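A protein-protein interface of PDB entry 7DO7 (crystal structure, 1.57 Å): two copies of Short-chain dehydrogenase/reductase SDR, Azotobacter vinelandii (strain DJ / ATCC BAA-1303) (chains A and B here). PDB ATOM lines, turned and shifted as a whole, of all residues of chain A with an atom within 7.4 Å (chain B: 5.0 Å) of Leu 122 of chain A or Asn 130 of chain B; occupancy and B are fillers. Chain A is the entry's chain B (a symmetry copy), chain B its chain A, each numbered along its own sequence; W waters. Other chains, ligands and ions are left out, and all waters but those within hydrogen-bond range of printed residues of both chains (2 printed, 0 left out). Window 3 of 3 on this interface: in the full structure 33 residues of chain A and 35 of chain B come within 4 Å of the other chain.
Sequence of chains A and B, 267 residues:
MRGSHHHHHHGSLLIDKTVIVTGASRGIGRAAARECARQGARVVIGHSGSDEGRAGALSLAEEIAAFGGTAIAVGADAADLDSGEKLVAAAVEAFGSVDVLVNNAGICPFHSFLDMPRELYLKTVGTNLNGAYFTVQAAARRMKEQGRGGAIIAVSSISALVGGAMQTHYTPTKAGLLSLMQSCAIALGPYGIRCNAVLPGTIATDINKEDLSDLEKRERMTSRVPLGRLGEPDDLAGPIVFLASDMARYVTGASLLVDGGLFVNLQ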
ATOM      1  N   ALA A  79     -11.695  36.564 -12.225  1.00  0.00           N
ATOM      2  CA  ALA A  79     -12.565  35.401 -12.369  1.00  0.00           C
ATOM      3  C   ALA A  79     -13.855  35.721 -13.121  1.00  0.00           C
ATOM      4  O   ALA A  79     -14.520  34.794 -13.598  1.00  0.00           O
ATOM      5  CB  ALA A  79     -12.891  34.819 -10.995  1.00  0.00           C
ATOM      6  N   ILE A 107      -4.162  33.501  -7.851  1.00  0.00           N
ATOM      7  CA  ILE A 107      -4.242  32.996  -6.489  1.00  0.00           C
ATOM      8  C   ILE A 107      -3.559  31.637  -6.421  1.00  0.00           C
ATOM      9  O   ILE A 107      -3.509  30.890  -7.404  1.00  0.00           O
ATOM     10  CB  ILE A 107      -5.705  32.896  -6.007  1.00  0.00           C
ATOM     11  CG1 ILE A 107      -6.485  31.860  -6.822  1.00  0.00           C
ATOM     12  CG2 ILE A 107      -6.372  34.260  -6.064  1.00  0.00           C
ATOM     13  CD1 ILE A 107      -7.875  31.576  -6.287  1.00  0.00           C
ATOM     14  N   MET A 116      -8.930  17.979  -2.265  1.00  0.00           N
ATOM     15  CA  MET A 116      -9.227  19.248  -2.922  1.00  0.00           C
ATOM     16  C   MET A 116     -10.726  19.387  -3.161  1.00  0.00           C
ATOM     17  O   MET A 116     -11.318  18.524  -3.824  1.00  0.00           O
ATOM     18  CB  MET A 116      -8.496  19.342  -4.258  1.00  0.00           C
ATOM     19  CG  MET A 116      -8.834  20.586  -5.037  1.00  0.00           C
ATOM     20  SD  MET A 116      -8.095  22.071  -4.328  1.00  0.00           S
ATOM     21  CE  MET A 116      -6.379  21.590  -4.315  1.00  0.00           C
ATOM     22  N   PRO A 117     -11.368  20.433  -2.657  1.00  0.00           N
ATOM     23  CA  PRO A 117     -12.780  20.653  -2.977  1.00  0.00           C
ATOM     24  C   PRO A 117     -12.948  21.284  -4.351  1.00  0.00           C
ATOM     25  O   PRO A 117     -12.114  22.065  -4.816  1.00  0.00           O
ATOM     26  CB  PRO A 117     -13.250  21.596  -1.863  1.00  0.00           C
ATOM     27  CG  PRO A 117     -12.016  22.326  -1.434  1.00  0.00           C
ATOM     28  CD  PRO A 117     -10.848  21.407  -1.674  1.00  0.00           C
ATOM     29  N   ARG A 118     -14.057  20.932  -5.005  1.00  0.00           N
ATOM     30  CA  ARG A 118     -14.266  21.392  -6.375  1.00  0.00           C
ATOM     31  C   ARG A 118     -14.366  22.908  -6.455  1.00  0.00           C
ATOM     32  O   ARG A 118     -13.893  23.510  -7.424  1.00  0.00           O
ATOM     33  CB  ARG A 118     -15.508  20.738  -6.965  1.00  0.00           C
ATOM     34  CG  ARG A 118     -15.357  19.250  -7.092  1.00  0.00           C
ATOM     35  CD  ARG A 118     -16.590  18.642  -7.690  1.00  0.00           C
ATOM     36  NE  ARG A 118     -16.575  17.195  -7.550  1.00  0.00           N
ATOM     37  CZ  ARG A 118     -17.634  16.431  -7.772  1.00  0.00           C
ATOM     38  NH1 ARG A 118     -18.775  16.985  -8.150  1.00  0.00           N
ATOM     39  NH2 ARG A 118     -17.548  15.117  -7.621  1.00  0.00           N
ATOM     40  N   GLU A 119     -14.970  23.550  -5.448  1.00  0.00           N
ATOM     41  CA  GLU A 119     -15.109  25.005  -5.491  1.00  0.00           C
ATOM     42  C   GLU A 119     -13.747  25.694  -5.490  1.00  0.00           C
ATOM     43  O   GLU A 119     -13.521  26.650  -6.245  1.00  0.00           O
ATOM     44  CB  GLU A 119     -15.951  25.494  -4.310  1.00  0.00           C
ATOM     45  N   LEU A 120     -12.828  25.229  -4.643  1.00  0.00           N
ATOM     46  CA  LEU A 120     -11.501  25.829  -4.601  1.00  0.00           C
ATOM     47  C   LEU A 120     -10.741  25.561  -5.893  1.00  0.00           C
ATOM     48  O   LEU A 120     -10.087  26.464  -6.433  1.00  0.00           O
ATOM     49  CB  LEU A 120     -10.721  25.298  -3.402  1.00  0.00           C
ATOM     50  CG  LEU A 120      -9.436  26.047  -3.048  1.00  0.00           C
ATOM     51  CD1 LEU A 120      -9.737  27.458  -2.564  1.00  0.00           C
ATOM     52  CD2 LEU A 120      -8.664  25.267  -1.996  1.00  0.00           C
ATOM     53  N   TYR A 121     -10.821  24.327  -6.404  1.00  0.00           N
ATOM     54  CA  TYR A 121     -10.188  24.036  -7.683  1.00  0.00           C
ATOM     55  C   TYR A 121     -10.732  24.958  -8.756  1.00  0.00           C
ATOM     56  O   TYR A 121      -9.974  25.599  -9.494  1.00  0.00           O
ATOM     57  CB  TYR A 121     -10.412  22.581  -8.097  1.00  0.00           C
ATOM     58  CG  TYR A 121      -9.932  22.337  -9.515  1.00  0.00           C
ATOM     59  CD1 TYR A 121      -8.607  21.998  -9.770  1.00  0.00           C
ATOM     60  CD2 TYR A 121     -10.796  22.471 -10.601  1.00  0.00           C
ATOM     61  CE1 TYR A 121      -8.151  21.809 -11.064  1.00  0.00           C
ATOM     62  CE2 TYR A 121     -10.355  22.271 -11.890  1.00  0.00           C
ATOM     63  CZ  TYR A 121      -9.032  21.941 -12.117  1.00  0.00           C
ATOM     64  OH  TYR A 121      -8.591  21.747 -13.405  1.00  0.00           O
ATOM     65  N   LEU A 122     -12.055  25.056  -8.835  1.00  0.00           N
ATOM     66  CA  LEU A 122     -12.658  25.788  -9.940  1.00  0.00           C
ATOM     67  C   LEU A 122     -12.375  27.282  -9.850  1.00  0.00           C
ATOM     68  O   LEU A 122     -12.284  27.961 -10.880  1.00  0.00           O
ATOM     69  CB  LEU A 122     -14.162  25.524  -9.982  1.00  0.00           C
ATOM     70  CG  LEU A 122     -14.588  24.158 -10.508  1.00  0.00           C
ATOM     71  CD1 LEU A 122     -16.105  24.010 -10.396  1.00  0.00           C
ATOM     72  CD2 LEU A 122     -14.116  23.952 -11.947  1.00  0.00           C
ATOM     73  N   LYS A 123     -12.216  27.814  -8.643  1.00  0.00           N
ATOM     74  CA  LYS A 123     -11.876  29.224  -8.525  1.00  0.00           C
ATOM     75  C   LYS A 123     -10.428  29.480  -8.917  1.00  0.00           C
ATOM     76  O   LYS A 123     -10.107  30.550  -9.445  1.00  0.00           O
ATOM     77  CB  LYS A 123     -12.138  29.709  -7.104  1.00  0.00           C
ATOM     78  CG  LYS A 123     -11.741  31.151  -6.885  1.00  0.00           C
ATOM     79  CD  LYS A 123     -12.048  31.602  -5.469  1.00  0.00           C
ATOM     80  CE  LYS A 123     -11.495  30.638  -4.431  1.00  0.00           C
ATOM     81  NZ  LYS A 123     -11.586  31.224  -3.063  1.00  0.00           N
ATOM     82  N   THR A 124      -9.546  28.513  -8.670  1.00  0.00           N
ATOM     83  CA  THR A 124      -8.147  28.679  -9.047  1.00  0.00           C
ATOM     84  C   THR A 124      -7.987  28.697 -10.560  1.00  0.00           C
ATOM     85  O   THR A 124      -7.297  29.558 -11.109  1.00  0.00           O
ATOM     86  CB  THR A 124      -7.311  27.561  -8.429  1.00  0.00           C
ATOM     87  OG1 THR A 124      -7.514  27.559  -7.005  1.00  0.00           O
ATOM     88  CG2 THR A 124      -5.836  27.789  -8.724  1.00  0.00           C
ATOM     89  N   VAL A 125      -8.623  27.750 -11.247  1.00  0.00           N
ATOM     90  CA  VAL A 125      -8.570  27.732 -12.705  1.00  0.00           C
ATOM     91  C   VAL A 125      -9.310  28.929 -13.298  1.00  0.00           C
ATOM     92  O   VAL A 125      -8.845  29.535 -14.270  1.00  0.00           O
ATOM     93  CB  VAL A 125      -9.101  26.382 -13.241  1.00  0.00           C
ATOM     94  CG1 VAL A 125     -10.597  26.235 -12.984  1.00  0.00           C
ATOM     95  CG2 VAL A 125      -8.803  26.242 -14.737  1.00  0.00           C
ATOM     96  N   GLY A 126     -10.441  29.316 -12.703  1.00  0.00           N
ATOM     97  CA  GLY A 126     -11.185  30.449 -13.230  1.00  0.00           C
ATOM     98  C   GLY A 126     -10.438  31.766 -13.120  1.00  0.00           C
ATOM     99  O   GLY A 126     -10.449  32.578 -14.050  1.00  0.00           O
ATOM    100  N   THR A 127      -9.799  32.007 -11.974  1.00  0.00           N
ATOM    101  CA  THR A 127      -9.034  33.233 -11.770  1.00  0.00           C
ATOM    102  C   THR A 127      -7.745  33.231 -12.588  1.00  0.00           C
ATOM    103  O   THR A 127      -7.442  34.195 -13.300  1.00  0.00           O
ATOM    104  CB  THR A 127      -8.715  33.377 -10.279  1.00  0.00           C
ATOM    105  OG1 THR A 127      -9.936  33.334  -9.527  1.00  0.00           O
ATOM    106  CG2 THR A 127      -7.976  34.676  -9.997  1.00  0.00           C
ATOM    107  N   ASN A 128      -6.979  32.144 -12.510  1.00  0.00           N
ATOM    108  CA  ASN A 128      -5.613  32.157 -13.022  1.00  0.00           C
ATOM    109  C   ASN A 128      -5.545  31.941 -14.520  1.00  0.00           C
ATOM    110  O   ASN A 128      -4.637  32.466 -15.172  1.00  0.00           O
ATOM    111  CB  ASN A 128      -4.785  31.069 -12.353  1.00  0.00           C
ATOM    112  CG  ASN A 128      -4.522  31.344 -10.884  1.00  0.00           C
ATOM    113  OD1 ASN A 128      -5.039  32.304 -10.310  1.00  0.00           O
ATOM    114  ND2 ASN A 128      -3.704  30.496 -10.266  1.00  0.00           N
ATOM    115  N   LEU A 129      -6.458  31.148 -15.060  1.00  0.00           N
ATOM    116  CA  LEU A 129      -6.370  30.724 -16.452  1.00  0.00           C
ATOM    117  C   LEU A 129      -7.549  31.190 -17.294  1.00  0.00           C
ATOM    118  O   LEU A 129      -7.330  31.825 -18.325  1.00  0.00           O
ATOM    119  CB  LEU A 129      -6.247  29.197 -16.527  1.00  0.00           C
ATOM    120  CG  LEU A 129      -6.066  28.728 -17.975  1.00  0.00           C
ATOM    121  CD1 LEU A 129      -4.765  29.276 -18.528  1.00  0.00           C
ATOM    122  CD2 LEU A 129      -6.100  27.208 -18.051  1.00  0.00           C
ATOM    123  N   ASN A 130      -8.787  30.878 -16.902  1.00  0.00           N
ATOM    124  CA  ASN A 130      -9.933  31.242 -17.729  1.00  0.00           C
ATOM    125  C   ASN A 130     -10.057  32.755 -17.855  1.00  0.00           C
ATOM    126  O   ASN A 130     -10.231  33.288 -18.957  1.00  0.00           O
ATOM    127  CB  ASN A 130     -11.208  30.629 -17.151  1.00  0.00           C
ATOM    128  CG  ASN A 130     -11.151  29.118 -17.104  1.00  0.00           C
ATOM    129  OD1 ASN A 130     -10.220  28.512 -17.629  1.00  0.00           O
ATOM    130  ND2 ASN A 130     -12.134  28.495 -16.460  1.00  0.00           N
ATOM    131  N   HIS A 169      -3.766  21.921  -8.109  1.00  0.00           N
ATOM    132  CA  HIS A 169      -4.748  22.785  -8.756  1.00  0.00           C
ATOM    133  C   HIS A 169      -4.129  24.018  -9.390  1.00  0.00           C
ATOM    134  O   HIS A 169      -4.754  24.638 -10.256  1.00  0.00           O
ATOM    135  CB  HIS A 169      -5.805  23.241  -7.744  1.00  0.00           C
ATOM    136  CG  HIS A 169      -5.238  23.919  -6.530  1.00  0.00           C
ATOM    137  ND1 HIS A 169      -4.133  23.446  -5.854  1.00  0.00           N
ATOM    138  CD2 HIS A 169      -5.638  25.029  -5.861  1.00  0.00           C
ATOM    139  CE1 HIS A 169      -3.870  24.240  -4.829  1.00  0.00           C
ATOM    140  NE2 HIS A 169      -4.772  25.205  -4.807  1.00  0.00           N
ATOM    141  N   LEU B  81     -17.802  16.354 -13.196  1.00  0.00           N
ATOM    142  CA  LEU B  81     -16.735  16.185 -12.217  1.00  0.00           C
ATOM    143  C   LEU B  81     -16.988  15.036 -11.247  1.00  0.00           C
ATOM    144  O   LEU B  81     -16.080  14.685 -10.485  1.00  0.00           O
ATOM    145  CB  LEU B  81     -16.521  17.489 -11.449  1.00  0.00           C
ATOM    146  CG  LEU B  81     -16.217  18.695 -12.341  1.00  0.00           C
ATOM    147  CD1 LEU B  81     -15.791  19.890 -11.494  1.00  0.00           C
ATOM    148  CD2 LEU B  81     -15.153  18.358 -13.381  1.00  0.00           C
ATOM    149  N   VAL B 125     -11.880  23.241 -21.483  1.00  0.00           N
ATOM    150  CA  VAL B 125     -11.197  23.129 -20.198  1.00  0.00           C
ATOM    151  C   VAL B 125     -11.918  22.135 -19.289  1.00  0.00           C
ATOM    152  O   VAL B 125     -11.280  21.348 -18.572  1.00  0.00           O
ATOM    153  CB  VAL B 125     -11.069  24.518 -19.547  1.00  0.00           C
ATOM    154  CG1 VAL B 125     -10.367  24.402 -18.193  1.00  0.00           C
ATOM    155  CG2 VAL B 125     -10.283  25.442 -20.440  1.00  0.00           C
ATOM    156  N   GLY B 126     -13.254  22.168 -19.276  1.00  0.00           N
ATOM    157  CA  GLY B 126     -13.991  21.265 -18.408  1.00  0.00           C
ATOM    158  C   GLY B 126     -13.782  19.804 -18.753  1.00  0.00           C
ATOM    159  O   GLY B 126     -13.617  18.963 -17.866  1.00  0.00           O
ATOM    160  N   ASN B 128     -11.245  18.441 -20.767  1.00  0.00           N
ATOM    161  CA  ASN B 128      -9.870  18.009 -20.960  1.00  0.00           C
ATOM    162  C   ASN B 128      -9.030  18.086 -19.708  1.00  0.00           C
ATOM    163  O   ASN B 128      -8.121  17.266 -19.542  1.00  0.00           O
ATOM    164  CB  ASN B 128      -9.184  18.868 -22.020  1.00  0.00           C
ATOM    165  CG  ASN B 128      -9.724  18.625 -23.399  1.00  0.00           C
ATOM    166  OD1 ASN B 128     -10.699  17.893 -23.574  1.00  0.00           O
ATOM    167  ND2 ASN B 128      -9.086  19.230 -24.388  1.00  0.00           N
ATOM    168  N   LEU B 129      -9.290  19.069 -18.846  1.00  0.00           N
ATOM    169  CA  LEU B 129      -8.453  19.316 -17.675  1.00  0.00           C
ATOM    170  C   LEU B 129      -9.221  19.146 -16.374  1.00  0.00           C
ATOM    171  O   LEU B 129      -8.795  18.360 -15.512  1.00  0.00           O
ATOM    172  CB  LEU B 129      -7.852  20.724 -17.766  1.00  0.00           C
ATOM    173  CG  LEU B 129      -6.931  21.109 -16.611  1.00  0.00           C
ATOM    174  CD1 LEU B 129      -5.761  20.139 -16.559  1.00  0.00           C
ATOM    175  CD2 LEU B 129      -6.449  22.556 -16.759  1.00  0.00           C
ATOM    176  N   ASN B 130     -10.337  19.860 -16.192  1.00  0.00           N
ATOM    177  CA  ASN B 130     -11.039  19.824 -14.907  1.00  0.00           C
ATOM    178  C   ASN B 130     -11.589  18.434 -14.604  1.00  0.00           C
ATOM    179  O   ASN B 130     -11.468  17.933 -13.475  1.00  0.00           O
ATOM    180  CB  ASN B 130     -12.175  20.847 -14.886  1.00  0.00           C
ATOM    181  CG  ASN B 130     -11.700  22.266 -15.139  1.00  0.00           C
ATOM    182  OD1 ASN B 130     -10.495  22.568 -15.084  1.00  0.00           O
ATOM    183  ND2 ASN B 130     -12.651  23.159 -15.416  1.00  0.00           N
ATOM    184  N   GLY B 131     -12.216  17.800 -15.597  1.00  0.00           N
ATOM    185  CA  GLY B 131     -12.690  16.440 -15.404  1.00  0.00           C
ATOM    186  C   GLY B 131     -11.558  15.460 -15.186  1.00  0.00           C
ATOM    187  O   GLY B 131     -11.670  14.532 -14.378  1.00  0.00           O
ATOM    188  N   ALA B 132     -10.441  15.664 -15.888  1.00  0.00           N
ATOM    189  CA  ALA B 132      -9.266  14.839 -15.648  1.00  0.00           C
ATOM    190  C   ALA B 132      -8.785  14.967 -14.207  1.00  0.00           C
ATOM    191  O   ALA B 132      -8.457  13.961 -13.575  1.00  0.00           O
ATOM    192  CB  ALA B 132      -8.155  15.218 -16.626  1.00  0.00           C
ATOM    193  N   TYR B 133      -8.734  16.196 -13.675  1.00  0.00           N
ATOM    194  CA  TYR B 133      -8.280  16.416 -12.305  1.00  0.00           C
ATOM    195  C   TYR B 133      -9.052  15.543 -11.324  1.00  0.00           C
ATOM    196  O   TYR B 133      -8.463  14.875 -10.473  1.00  0.00           O
ATOM    197  CB  TYR B 133      -8.424  17.894 -11.934  1.00  0.00           C
ATOM    198  CG  TYR B 133      -7.852  18.263 -10.574  1.00  0.00           C
ATOM    199  CD1 TYR B 133      -8.607  18.115  -9.404  1.00  0.00           C
ATOM    200  CD2 TYR B 133      -6.556  18.758 -10.459  1.00  0.00           C
ATOM    201  CE1 TYR B 133      -8.083  18.457  -8.159  1.00  0.00           C
ATOM    202  CE2 TYR B 133      -6.016  19.096  -9.214  1.00  0.00           C
ATOM    203  CZ  TYR B 133      -6.789  18.952  -8.066  1.00  0.00           C
ATOM    204  OH  TYR B 133      -6.271  19.286  -6.829  1.00  0.00           O
ATOM    205  N   PHE B 134     -10.376  15.525 -11.436  1.00  0.00           N
ATOM    206  CA  PHE B 134     -11.157  14.784 -10.459  1.00  0.00           C
ATOM    207  C   PHE B 134     -11.296  13.305 -10.792  1.00  0.00           C
ATOM    208  O   PHE B 134     -11.547  12.505  -9.881  1.00  0.00           O
ATOM    209  CB  PHE B 134     -12.509  15.482 -10.265  1.00  0.00           C
ATOM    210  CG  PHE B 134     -12.368  16.801  -9.561  1.00  0.00           C
ATOM    211  CD1 PHE B 134     -12.102  16.848  -8.194  1.00  0.00           C
ATOM    212  CD2 PHE B 134     -12.376  17.984 -10.270  1.00  0.00           C
ATOM    213  CE1 PHE B 134     -11.923  18.053  -7.550  1.00  0.00           C
ATOM    214  CE2 PHE B 134     -12.200  19.199  -9.626  1.00  0.00           C
ATOM    215  CZ  PHE B 134     -11.966  19.233  -8.264  1.00  0.00           C
HETATM  216  O   HOH W   1     -15.167  15.013  -7.272  1.00  0.00           O
HETATM  217  O   HOH W   2     -13.074  26.063 -15.569  1.00  0.00           O
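The side-chain amide oxygen (OD1) of Asn 130 of chain B is in hydrogen-bond range of the side-chain hydroxyl (OH) of Tyr 121 of chain A, at 2.7 Å. The backbone carbonyl oxygen (O) of Leu 81 of chain B sits at hydrogen-bond distance from the guanidinium group (NH2) of Arg 118 of chain A (3.2 Å).
The backbone NH (N) of Asn 130 of chain B sits at hydrogen-bond distance from the backbone carbonyl oxygen (O) of Val 125 of chain B (3.0 Å).
Among the printed residues, pairs that only touch across the chains: Met 116 of chain A with Tyr 133 of chain B (3.4 Å), Tyr 121 of chain A with Tyr 133 of chain B (3.5 Å), Arg 118 of chain A with Phe 134 of chain B (3.6 Å), Tyr 121 of chain A with Leu 129 of chain B (3.7 Å), Tyr 121 of chain A with Phe 134 of chain B (3.7 Å), His 169 of chain A with Tyr 133 of chain B (3.8 Å), Met 116 of chain A with Phe 134 of chain B (3.8 Å) and Leu 122 of chain A with Asn 130 of chain B (3.8 Å).
Of the printed residues of chain B, Arg 118 of chain A touches Leu 81 and Phe 134. Of the printed residues of chain B, His 169 of chain A touches Tyr 133 (3.8 Å). Of the printed residues of chain A, Leu 81 of chain B touches Arg 118. Asn 130 of chain B touches just these residues of chain A: Tyr 121 (2.7 Å) and Leu 122 (3.8 Å). Printed residues of chain A within 4 Å of Tyr 133 of chain B: Met 116, Tyr 121 and His 169. The nearest printed residue of chain B that does not touch Arg 118 of chain A is Tyr 133 of chain B (7.1 Å).
Hydrophobic or aromatic side chains of chain B within 4 Å of the printed part of chain A: Leu 81, Leu 129, Tyr 133 and Phe 134. Of the 18 printed residues of chain A, 5 touch a printed residue of chain B. Along chain A the printed residues that touch a printed residue of chain B span positions 116 to 169. Among the printed residues, no Asp or Glu carboxylate lies within 4 Å of a Lys or Arg side-chain nitrogen of the other chain.
5 positions are printed for both chains. Of the 10 pairs that touch across the chains among the printed residues, none has its exchanged pair printed and touching as well.
Water W1 bridges the guanidinium group of Arg 118 of chain A and the backbone carbonyl oxygen of Leu 81 of chain B. Water W2 lies within hydrogen-bond range of the side-chain amide nitrogen of Asn 130 of chain A (2.8 Å) and the side-chain amide nitrogen of Asn 130 of chain B (2.9 Å).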
